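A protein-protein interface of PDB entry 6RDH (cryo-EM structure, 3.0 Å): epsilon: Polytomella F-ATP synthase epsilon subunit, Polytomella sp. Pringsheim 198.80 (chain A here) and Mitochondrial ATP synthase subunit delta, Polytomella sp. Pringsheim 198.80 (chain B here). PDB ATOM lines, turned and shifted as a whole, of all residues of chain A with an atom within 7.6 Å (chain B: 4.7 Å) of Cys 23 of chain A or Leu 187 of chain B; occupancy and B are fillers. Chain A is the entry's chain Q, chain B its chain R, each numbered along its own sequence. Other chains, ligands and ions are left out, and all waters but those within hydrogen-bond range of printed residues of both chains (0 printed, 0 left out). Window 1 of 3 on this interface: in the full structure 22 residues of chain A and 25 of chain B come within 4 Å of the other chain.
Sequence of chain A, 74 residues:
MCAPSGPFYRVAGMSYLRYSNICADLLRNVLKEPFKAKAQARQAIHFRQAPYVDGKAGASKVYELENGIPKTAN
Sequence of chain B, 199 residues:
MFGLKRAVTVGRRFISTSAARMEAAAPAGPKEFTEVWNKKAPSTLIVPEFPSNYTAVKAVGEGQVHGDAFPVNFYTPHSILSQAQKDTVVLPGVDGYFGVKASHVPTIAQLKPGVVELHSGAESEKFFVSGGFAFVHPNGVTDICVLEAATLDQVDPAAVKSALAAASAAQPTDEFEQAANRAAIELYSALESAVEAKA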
ATOM      1  N   PHE A   8      24.348  15.698  15.292  1.00  0.00           N
ATOM      2  CA  PHE A   8      23.527  16.902  15.377  1.00  0.00           C
ATOM      3  C   PHE A   8      24.294  18.096  15.924  1.00  0.00           C
ATOM      4  O   PHE A   8      23.941  19.241  15.628  1.00  0.00           O
ATOM      5  CB  PHE A   8      22.279  16.639  16.221  1.00  0.00           C
ATOM      6  CG  PHE A   8      22.551  16.396  17.677  1.00  0.00           C
ATOM      7  CD1 PHE A   8      22.417  17.417  18.603  1.00  0.00           C
ATOM      8  CD2 PHE A   8      22.887  15.136  18.130  1.00  0.00           C
ATOM      9  CE1 PHE A   8      22.656  17.195  19.936  1.00  0.00           C
ATOM     10  CE2 PHE A   8      23.121  14.908  19.465  1.00  0.00           C
ATOM     11  CZ  PHE A   8      23.001  15.939  20.367  1.00  0.00           C
ATOM     12  N   TYR A   9      25.332  17.860  16.721  1.00  0.00           N
ATOM     13  CA  TYR A   9      26.195  18.963  17.113  1.00  0.00           C
ATOM     14  C   TYR A   9      27.059  19.419  15.949  1.00  0.00           C
ATOM     15  O   TYR A   9      27.328  20.614  15.814  1.00  0.00           O
ATOM     16  CB  TYR A   9      27.062  18.567  18.305  1.00  0.00           C
ATOM     17  CG  TYR A   9      27.703  17.206  18.213  1.00  0.00           C
ATOM     18  CD1 TYR A   9      27.100  16.098  18.782  1.00  0.00           C
ATOM     19  CD2 TYR A   9      28.925  17.035  17.587  1.00  0.00           C
ATOM     20  CE1 TYR A   9      27.682  14.863  18.710  1.00  0.00           C
ATOM     21  CE2 TYR A   9      29.513  15.802  17.511  1.00  0.00           C
ATOM     22  CZ  TYR A   9      28.888  14.722  18.073  1.00  0.00           C
ATOM     23  OH  TYR A   9      29.471  13.485  18.001  1.00  0.00           O
ATOM     24  N   TYR A  16      32.856  18.796  18.705  1.00  0.00           N
ATOM     25  CA  TYR A  16      32.563  17.736  19.657  1.00  0.00           C
ATOM     26  C   TYR A  16      32.981  18.138  21.059  1.00  0.00           C
ATOM     27  O   TYR A  16      32.315  17.778  22.034  1.00  0.00           O
ATOM     28  CB  TYR A  16      33.247  16.436  19.268  1.00  0.00           C
ATOM     29  CG  TYR A  16      33.045  15.385  20.321  1.00  0.00           C
ATOM     30  CD1 TYR A  16      31.788  14.873  20.571  1.00  0.00           C
ATOM     31  CD2 TYR A  16      34.096  14.949  21.104  1.00  0.00           C
ATOM     32  CE1 TYR A  16      31.587  13.933  21.543  1.00  0.00           C
ATOM     33  CE2 TYR A  16      33.902  14.015  22.081  1.00  0.00           C
ATOM     34  CZ  TYR A  16      32.647  13.510  22.293  1.00  0.00           C
ATOM     35  OH  TYR A  16      32.454  12.569  23.267  1.00  0.00           O
ATOM     36  N   LEU A  17      34.083  18.880  21.172  1.00  0.00           N
ATOM     37  CA  LEU A  17      34.571  19.319  22.473  1.00  0.00           C
ATOM     38  C   LEU A  17      33.572  20.225  23.163  1.00  0.00           C
ATOM     39  O   LEU A  17      33.308  20.066  24.358  1.00  0.00           O
ATOM     40  CB  LEU A  17      35.894  20.048  22.313  1.00  0.00           C
ATOM     41  CG  LEU A  17      37.114  19.179  22.113  1.00  0.00           C
ATOM     42  CD1 LEU A  17      38.207  20.085  21.696  1.00  0.00           C
ATOM     43  CD2 LEU A  17      37.450  18.499  23.407  1.00  0.00           C
ATOM     44  N   ARG A  18      32.984  21.159  22.418  1.00  0.00           N
ATOM     45  CA  ARG A  18      32.034  22.074  23.025  1.00  0.00           C
ATOM     46  C   ARG A  18      30.747  21.363  23.389  1.00  0.00           C
ATOM     47  O   ARG A  18      30.152  21.654  24.427  1.00  0.00           O
ATOM     48  CB  ARG A  18      31.742  23.240  22.098  1.00  0.00           C
ATOM     49  CG  ARG A  18      31.065  24.364  22.826  1.00  0.00           C
ATOM     50  CD  ARG A  18      30.759  25.497  21.910  1.00  0.00           C
ATOM     51  NE  ARG A  18      31.942  26.193  21.441  1.00  0.00           N
ATOM     52  CZ  ARG A  18      32.473  27.231  22.067  1.00  0.00           C
ATOM     53  NH1 ARG A  18      31.921  27.678  23.182  1.00  0.00           N
ATOM     54  NH2 ARG A  18      33.551  27.823  21.576  1.00  0.00           N
ATOM     55  N   TYR A  19      30.330  20.394  22.574  1.00  0.00           N
ATOM     56  CA  TYR A  19      29.131  19.619  22.874  1.00  0.00           C
ATOM     57  C   TYR A  19      29.318  18.775  24.125  1.00  0.00           C
ATOM     58  O   TYR A  19      28.465  18.774  25.023  1.00  0.00           O
ATOM     59  CB  TYR A  19      28.780  18.740  21.676  1.00  0.00           C
ATOM     60  CG  TYR A  19      27.996  17.501  22.025  1.00  0.00           C
ATOM     61  CD1 TYR A  19      28.601  16.250  22.033  1.00  0.00           C
ATOM     62  CD2 TYR A  19      26.651  17.580  22.334  1.00  0.00           C
ATOM     63  CE1 TYR A  19      27.892  15.125  22.356  1.00  0.00           C
ATOM     64  CE2 TYR A  19      25.934  16.459  22.651  1.00  0.00           C
ATOM     65  CZ  TYR A  19      26.558  15.235  22.663  1.00  0.00           C
ATOM     66  OH  TYR A  19      25.845  14.106  22.982  1.00  0.00           O
ATOM     67  N   SER A  20      30.441  18.065  24.205  1.00  0.00           N
ATOM     68  CA  SER A  20      30.696  17.202  25.345  1.00  0.00           C
ATOM     69  C   SER A  20      30.944  18.005  26.606  1.00  0.00           C
ATOM     70  O   SER A  20      30.588  17.561  27.700  1.00  0.00           O
ATOM     71  CB  SER A  20      31.878  16.294  25.046  1.00  0.00           C
ATOM     72  OG  SER A  20      31.926  15.225  25.966  1.00  0.00           O
ATOM     73  N   ASN A  21      31.499  19.210  26.479  1.00  0.00           N
ATOM     74  CA  ASN A  21      31.671  20.045  27.656  1.00  0.00           C
ATOM     75  C   ASN A  21      30.379  20.727  28.064  1.00  0.00           C
ATOM     76  O   ASN A  21      30.197  21.013  29.247  1.00  0.00           O
ATOM     77  CB  ASN A  21      32.767  21.069  27.413  1.00  0.00           C
ATOM     78  CG  ASN A  21      34.129  20.521  27.717  1.00  0.00           C
ATOM     79  OD1 ASN A  21      34.515  20.412  28.875  1.00  0.00           O
ATOM     80  ND2 ASN A  21      34.867  20.162  26.682  1.00  0.00           N
ATOM     81  N   ILE A  22      29.472  20.973  27.117  1.00  0.00           N
ATOM     82  CA  ILE A  22      28.125  21.413  27.465  1.00  0.00           C
ATOM     83  C   ILE A  22      27.409  20.337  28.264  1.00  0.00           C
ATOM     84  O   ILE A  22      26.789  20.623  29.293  1.00  0.00           O
ATOM     85  CB  ILE A  22      27.356  21.806  26.189  1.00  0.00           C
ATOM     86  CG1 ILE A  22      27.699  23.235  25.787  1.00  0.00           C
ATOM     87  CG2 ILE A  22      25.858  21.680  26.369  1.00  0.00           C
ATOM     88  CD1 ILE A  22      27.276  23.582  24.396  1.00  0.00           C
ATOM     89  N   CYS A  23      27.524  19.078  27.834  1.00  0.00           N
ATOM     90  CA  CYS A  23      26.919  17.994  28.606  1.00  0.00           C
ATOM     91  C   CYS A  23      27.611  17.788  29.947  1.00  0.00           C
ATOM     92  O   CYS A  23      26.949  17.428  30.926  1.00  0.00           O
ATOM     93  CB  CYS A  23      26.915  16.686  27.820  1.00  0.00           C
ATOM     94  SG  CYS A  23      26.205  16.765  26.185  1.00  0.00           S
ATOM     95  N   ALA A  24      28.920  18.017  30.025  1.00  0.00           N
ATOM     96  CA  ALA A  24      29.612  17.900  31.305  1.00  0.00           C
ATOM     97  C   ALA A  24      29.174  18.994  32.271  1.00  0.00           C
ATOM     98  O   ALA A  24      28.887  18.720  33.442  1.00  0.00           O
ATOM     99  CB  ALA A  24      31.120  17.948  31.087  1.00  0.00           C
ATOM    100  N   ASP A  25      29.089  20.236  31.787  1.00  0.00           N
ATOM    101  CA  ASP A  25      28.623  21.340  32.618  1.00  0.00           C
ATOM    102  C   ASP A  25      27.163  21.169  33.002  1.00  0.00           C
ATOM    103  O   ASP A  25      26.749  21.599  34.081  1.00  0.00           O
ATOM    104  CB  ASP A  25      28.813  22.672  31.893  1.00  0.00           C
ATOM    105  CG  ASP A  25      30.275  22.999  31.639  1.00  0.00           C
ATOM    106  OD1 ASP A  25      31.141  22.495  32.382  1.00  0.00           O
ATOM    107  OD2 ASP A  25      30.560  23.762  30.693  1.00  0.00           O
ATOM    108  N   LEU A  26      26.383  20.506  32.160  1.00  0.00           N
ATOM    109  CA  LEU A  26      24.984  20.273  32.476  1.00  0.00           C
ATOM    110  C   LEU A  26      24.808  19.142  33.474  1.00  0.00           C
ATOM    111  O   LEU A  26      23.854  19.163  34.256  1.00  0.00           O
ATOM    112  CB  LEU A  26      24.224  19.990  31.188  1.00  0.00           C
ATOM    113  CG  LEU A  26      23.416  21.101  30.545  1.00  0.00           C
ATOM    114  CD1 LEU A  26      24.171  22.390  30.541  1.00  0.00           C
ATOM    115  CD2 LEU A  26      23.177  20.691  29.134  1.00  0.00           C
ATOM    116  N   LEU A  27      25.699  18.152  33.463  1.00  0.00           N
ATOM    117  CA  LEU A  27      25.719  17.189  34.557  1.00  0.00           C
ATOM    118  C   LEU A  27      26.166  17.845  35.854  1.00  0.00           C
ATOM    119  O   LEU A  27      25.680  17.483  36.929  1.00  0.00           O
ATOM    120  CB  LEU A  27      26.633  16.015  34.221  1.00  0.00           C
ATOM    121  CG  LEU A  27      26.699  14.884  35.247  1.00  0.00           C
ATOM    122  CD1 LEU A  27      25.307  14.429  35.601  1.00  0.00           C
ATOM    123  CD2 LEU A  27      27.509  13.720  34.752  1.00  0.00           C
ATOM    124  N   ARG A  28      27.072  18.818  35.776  1.00  0.00           N
ATOM    125  CA  ARG A  28      27.506  19.506  36.986  1.00  0.00           C
ATOM    126  C   ARG A  28      26.439  20.444  37.541  1.00  0.00           C
ATOM    127  O   ARG A  28      26.334  20.599  38.760  1.00  0.00           O
ATOM    128  CB  ARG A  28      28.791  20.285  36.716  1.00  0.00           C
ATOM    129  CG  ARG A  28      29.991  19.417  36.439  1.00  0.00           C
ATOM    130  CD  ARG A  28      31.225  20.259  36.244  1.00  0.00           C
ATOM    131  NE  ARG A  28      32.275  19.508  35.575  1.00  0.00           N
ATOM    132  CZ  ARG A  28      32.694  19.764  34.345  1.00  0.00           C
ATOM    133  NH1 ARG A  28      32.157  20.756  33.657  1.00  0.00           N
ATOM    134  NH2 ARG A  28      33.652  19.029  33.804  1.00  0.00           N
ATOM    135  N   ASN A  29      25.633  21.061  36.681  1.00  0.00           N
ATOM    136  CA  ASN A  29      24.645  22.038  37.125  1.00  0.00           C
ATOM    137  C   ASN A  29      23.431  21.421  37.808  1.00  0.00           C
ATOM    138  O   ASN A  29      22.557  22.168  38.254  1.00  0.00           O
ATOM    139  CB  ASN A  29      24.166  22.883  35.942  1.00  0.00           C
ATOM    140  CG  ASN A  29      25.149  23.967  35.563  1.00  0.00           C
ATOM    141  OD1 ASN A  29      25.405  24.201  34.384  1.00  0.00           O
ATOM    142  ND2 ASN A  29      25.705  24.638  36.563  1.00  0.00           N
ATOM    143  N   VAL A  30      23.326  20.094  37.870  1.00  0.00           N
ATOM    144  CA  VAL A  30      22.258  19.426  38.608  1.00  0.00           C
ATOM    145  C   VAL A  30      22.876  18.418  39.563  1.00  0.00           C
ATOM    146  O   VAL A  30      22.228  17.454  39.985  1.00  0.00           O
ATOM    147  CB  VAL A  30      21.239  18.752  37.671  1.00  0.00           C
ATOM    148  CG1 VAL A  30      20.514  19.791  36.834  1.00  0.00           C
ATOM    149  CG2 VAL A  30      21.932  17.754  36.761  1.00  0.00           C
ATOM    150  N   ILE A  69      31.471  26.493  29.858  1.00  0.00           N
ATOM    151  CA  ILE A  69      31.740  26.734  28.446  1.00  0.00           C
ATOM    152  C   ILE A  69      30.515  27.461  27.898  1.00  0.00           C
ATOM    153  O   ILE A  69      29.418  27.308  28.461  1.00  0.00           O
ATOM    154  CB  ILE A  69      32.071  25.401  27.739  1.00  0.00           C
ATOM    155  CG1 ILE A  69      32.947  25.596  26.502  1.00  0.00           C
ATOM    156  CG2 ILE A  69      30.825  24.623  27.382  1.00  0.00           C
ATOM    157  CD1 ILE A  69      33.693  24.368  26.078  1.00  0.00           C
ATOM    158  N   PRO B 113      24.909   9.873  27.048  1.00  0.00           N
ATOM    159  CA  PRO B 113      24.710  10.057  28.491  1.00  0.00           C
ATOM    160  C   PRO B 113      23.947   8.923  29.152  1.00  0.00           C
ATOM    161  O   PRO B 113      22.768   8.708  28.868  1.00  0.00           O
ATOM    162  CB  PRO B 113      23.914  11.358  28.555  1.00  0.00           C
ATOM    163  CG  PRO B 113      24.410  12.123  27.423  1.00  0.00           C
ATOM    164  CD  PRO B 113      24.758  11.150  26.332  1.00  0.00           C
ATOM    165  N   PHE B 128      27.236   7.286  36.488  1.00  0.00           N
ATOM    166  CA  PHE B 128      26.537   7.998  35.430  1.00  0.00           C
ATOM    167  C   PHE B 128      27.521   8.917  34.722  1.00  0.00           C
ATOM    168  O   PHE B 128      28.000   9.887  35.311  1.00  0.00           O
ATOM    169  CB  PHE B 128      25.370   8.806  35.986  1.00  0.00           C
ATOM    170  CG  PHE B 128      24.603   9.547  34.938  1.00  0.00           C
ATOM    171  CD1 PHE B 128      23.674   8.891  34.158  1.00  0.00           C
ATOM    172  CD2 PHE B 128      24.807  10.898  34.728  1.00  0.00           C
ATOM    173  CE1 PHE B 128      22.970   9.563  33.187  1.00  0.00           C
ATOM    174  CE2 PHE B 128      24.108  11.570  33.755  1.00  0.00           C
ATOM    175  CZ  PHE B 128      23.187  10.903  32.989  1.00  0.00           C
ATOM    176  N   SER B 130      28.486  11.488  31.371  1.00  0.00           N
ATOM    177  CA  SER B 130      27.784  12.495  30.599  1.00  0.00           C
ATOM    178  C   SER B 130      28.060  12.392  29.110  1.00  0.00           C
ATOM    179  O   SER B 130      27.755  13.327  28.367  1.00  0.00           O
ATOM    180  CB  SER B 130      28.150  13.883  31.095  1.00  0.00           C
ATOM    181  OG  SER B 130      27.279  14.820  30.516  1.00  0.00           O
ATOM    182  N   ALA B 183      20.911  18.240  23.578  1.00  0.00           N
ATOM    183  CA  ALA B 183      21.839  17.602  24.508  1.00  0.00           C
ATOM    184  C   ALA B 183      21.349  17.719  25.942  1.00  0.00           C
ATOM    185  O   ALA B 183      21.452  16.763  26.721  1.00  0.00           O
ATOM    186  CB  ALA B 183      23.225  18.218  24.369  1.00  0.00           C
ATOM    187  N   ALA B 184      20.759  18.870  26.282  1.00  0.00           N
ATOM    188  CA  ALA B 184      20.202  19.088  27.611  1.00  0.00           C
ATOM    189  C   ALA B 184      19.059  18.133  27.904  1.00  0.00           C
ATOM    190  O   ALA B 184      19.032  17.492  28.961  1.00  0.00           O
ATOM    191  CB  ALA B 184      19.728  20.532  27.740  1.00  0.00           C
ATOM    192  N   ILE B 185      18.106  18.020  26.974  1.00  0.00           N
ATOM    193  CA  ILE B 185      16.931  17.205  27.253  1.00  0.00           C
ATOM    194  C   ILE B 185      17.286  15.728  27.240  1.00  0.00           C
ATOM    195  O   ILE B 185      16.771  14.964  28.060  1.00  0.00           O
ATOM    196  CB  ILE B 185      15.762  17.527  26.299  1.00  0.00           C
ATOM    197  CG1 ILE B 185      16.101  17.248  24.837  1.00  0.00           C
ATOM    198  CG2 ILE B 185      15.314  18.956  26.477  1.00  0.00           C
ATOM    199  CD1 ILE B 185      14.905  17.288  23.928  1.00  0.00           C
ATOM    200  N   GLU B 186      18.235  15.311  26.391  1.00  0.00           N
ATOM    201  CA  GLU B 186      18.587  13.898  26.396  1.00  0.00           C
ATOM    202  C   GLU B 186      19.416  13.539  27.623  1.00  0.00           C
ATOM    203  O   GLU B 186      19.212  12.465  28.201  1.00  0.00           O
ATOM    204  CB  GLU B 186      19.283  13.505  25.086  1.00  0.00           C
ATOM    205  CG  GLU B 186      20.748  13.846  24.945  1.00  0.00           C
ATOM    206  CD  GLU B 186      21.408  13.084  23.819  1.00  0.00           C
ATOM    207  OE1 GLU B 186      22.652  12.990  23.809  1.00  0.00           O
ATOM    208  OE2 GLU B 186      20.683  12.572  22.943  1.00  0.00           O
ATOM    209  N   LEU B 187      20.249  14.464  28.113  1.00  0.00           N
ATOM    210  CA  LEU B 187      21.041  14.175  29.299  1.00  0.00           C
ATOM    211  C   LEU B 187      20.170  14.147  30.547  1.00  0.00           C
ATOM    212  O   LEU B 187      20.237  13.199  31.336  1.00  0.00           O
ATOM    213  CB  LEU B 187      22.158  15.202  29.441  1.00  0.00           C
ATOM    214  CG  LEU B 187      22.846  15.267  30.798  1.00  0.00           C
ATOM    215  CD1 LEU B 187      23.623  14.011  31.094  1.00  0.00           C
ATOM    216  CD2 LEU B 187      23.763  16.423  30.791  1.00  0.00           C
ATOM    217  N   TYR B 188      19.329  15.168  30.731  1.00  0.00           N
ATOM    218  CA  TYR B 188      18.475  15.205  31.910  1.00  0.00           C
ATOM    219  C   TYR B 188      17.410  14.119  31.869  1.00  0.00           C
ATOM    220  O   TYR B 188      17.041  13.589  32.921  1.00  0.00           O
ATOM    221  CB  TYR B 188      17.815  16.572  32.041  1.00  0.00           C
ATOM    222  CG  TYR B 188      18.749  17.714  32.336  1.00  0.00           C
ATOM    223  CD1 TYR B 188      19.835  17.555  33.184  1.00  0.00           C
ATOM    224  CD2 TYR B 188      18.540  18.959  31.760  1.00  0.00           C
ATOM    225  CE1 TYR B 188      20.684  18.609  33.444  1.00  0.00           C
ATOM    226  CE2 TYR B 188      19.383  20.013  32.012  1.00  0.00           C
ATOM    227  CZ  TYR B 188      20.446  19.836  32.858  1.00  0.00           C
ATOM    228  OH  TYR B 188      21.279  20.899  33.109  1.00  0.00           O
ATOM    229  N   SER B 189      16.934  13.741  30.676  1.00  0.00           N
ATOM    230  CA  SER B 189      15.951  12.672  30.581  1.00  0.00           C
ATOM    231  C   SER B 189      16.575  11.318  30.879  1.00  0.00           C
ATOM    232  O   SER B 189      15.953  10.483  31.543  1.00  0.00           O
ATOM    233  CB  SER B 189      15.313  12.671  29.198  1.00  0.00           C
ATOM    234  OG  SER B 189      16.269  12.354  28.210  1.00  0.00           O
ATOM    235  N   ALA B 190      17.812  11.085  30.424  1.00  0.00           N
ATOM    236  CA  ALA B 190      18.497   9.856  30.808  1.00  0.00           C
ATOM    237  C   ALA B 190      18.835   9.849  32.290  1.00  0.00           C
ATOM    238  O   ALA B 190      18.842   8.787  32.922  1.00  0.00           O
ATOM    239  CB  ALA B 190      19.762   9.673  29.976  1.00  0.00           C
ATOM    240  N   LEU B 191      19.064  11.029  32.866  1.00  0.00           N
ATOM    241  CA  LEU B 191      19.372  11.114  34.285  1.00  0.00           C
ATOM    242  C   LEU B 191      18.145  10.828  35.141  1.00  0.00           C
ATOM    243  O   LEU B 191      18.247  10.142  36.161  1.00  0.00           O
ATOM    244  CB  LEU B 191      19.952  12.489  34.595  1.00  0.00           C
ATOM    245  CG  LEU B 191      20.636  12.686  35.936  1.00  0.00           C
ATOM    246  CD1 LEU B 191      21.492  11.483  36.306  1.00  0.00           C
ATOM    247  CD2 LEU B 191      21.476  13.929  35.831  1.00  0.00           C
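OH of Tyr 19 of chain A sits at hydrogen-bond distance from OE1 of Glu 186 of chain B (3.5 Å).
OG of Ser 130 of chain B lies within hydrogen-bond range of O of Cys 23 of chain A, at 2.7 Å.
OH of Tyr 188 of chain B is in hydrogen-bond range of O of Leu 26 of chain A (3.3 Å).
SG of Cys 23 of chain A is in hydrogen-bond range of O of Tyr 19 of chain A.
The backbone carbonyl oxygen (O) of Glu 186 of chain B lies within hydrogen-bond range of the side-chain hydroxyl (OG) of Ser 189 of chain B (2.9 Å).
Ala 183 of chain B touches Tyr 19 of chain A.
Cys 23 of chain A touches Ala 183 of chain B (SG to CB, 3.8 Å).
Leu 187 of chain B touches Cys 23 of chain A (CD2 to O, 3.3 Å).
Ala 184 of chain B touches Leu 26 of chain A.
CD2 of Leu 187 of chain B touches CB of Leu 26 of chain A, at 3.6 Å.
CD2 of Leu 27 of chain A touches CB of Ser 130 of chain B, at 3.7 Å.
Leu 27 of chain A touches Leu 187 of chain B.
Leu 27 of chain A touches Leu 191 of chain B (CD1 to CD2, 3.9 Å).
Tyr 188 of chain B touches Val 30 of chain A.
Val 30 of chain A touches Leu 191 of chain B.
Tyr 9 of chain A touches none of the printed residues of chain B.
Leu 17 of chain A touches none of the printed residues of chain B.
Of chain B, only Ser 130 (2.7 Å), Ala 183 (3.8 Å) and Leu 187 (3.3 Å) come within 4 Å of Cys 23 of chain A.
Printed residues of chain B within 4 Å of Leu 27 of chain A: Phe 128, Ser 130, Leu 187 and Leu 191.
Printed residues of chain A within 4 Å of Phe 128 of chain B: Leu 27 (3.6 Å).
Leu 187 of chain B touches three residues of chain A.
Of the printed residues of chain A, Leu 191 of chain B touches Leu 27 and Val 30.
The nearest printed residue of chain B that does not touch Cys 23 of chain A is Pro 113 of chain B (5.1 Å).
The nearest residue of chain A that does not touch Leu 187 of chain B is Ile 22 of chain A (5.4 Å).
The nearest printed residue of chain A that does not touch Ala 184 of chain B is Ile 22 of chain A (5.8 Å).
Hydrophobic or aromatic side chains of chain B that line the printed part of chain A: Phe 128, Ala 183, Ala 184, Leu 187, Tyr 188 and Leu 191.
Along chain B the printed residues that touch a printed residue of chain A span positions 128 to 191.
Of the 18 printed residues of chain A, 6 touch a printed residue of chain B.
Hydrophobic or aromatic side chains of chain A that line the printed part of chain B: Tyr 19, Leu 26, Leu 27 and Val 30.
Among the printed residues, 15 pairs touch across the chains.
Among the printed residues, no Asp or Glu carboxylate lies within 4 Å of a Lys or Arg side-chain nitrogen of the other chain.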
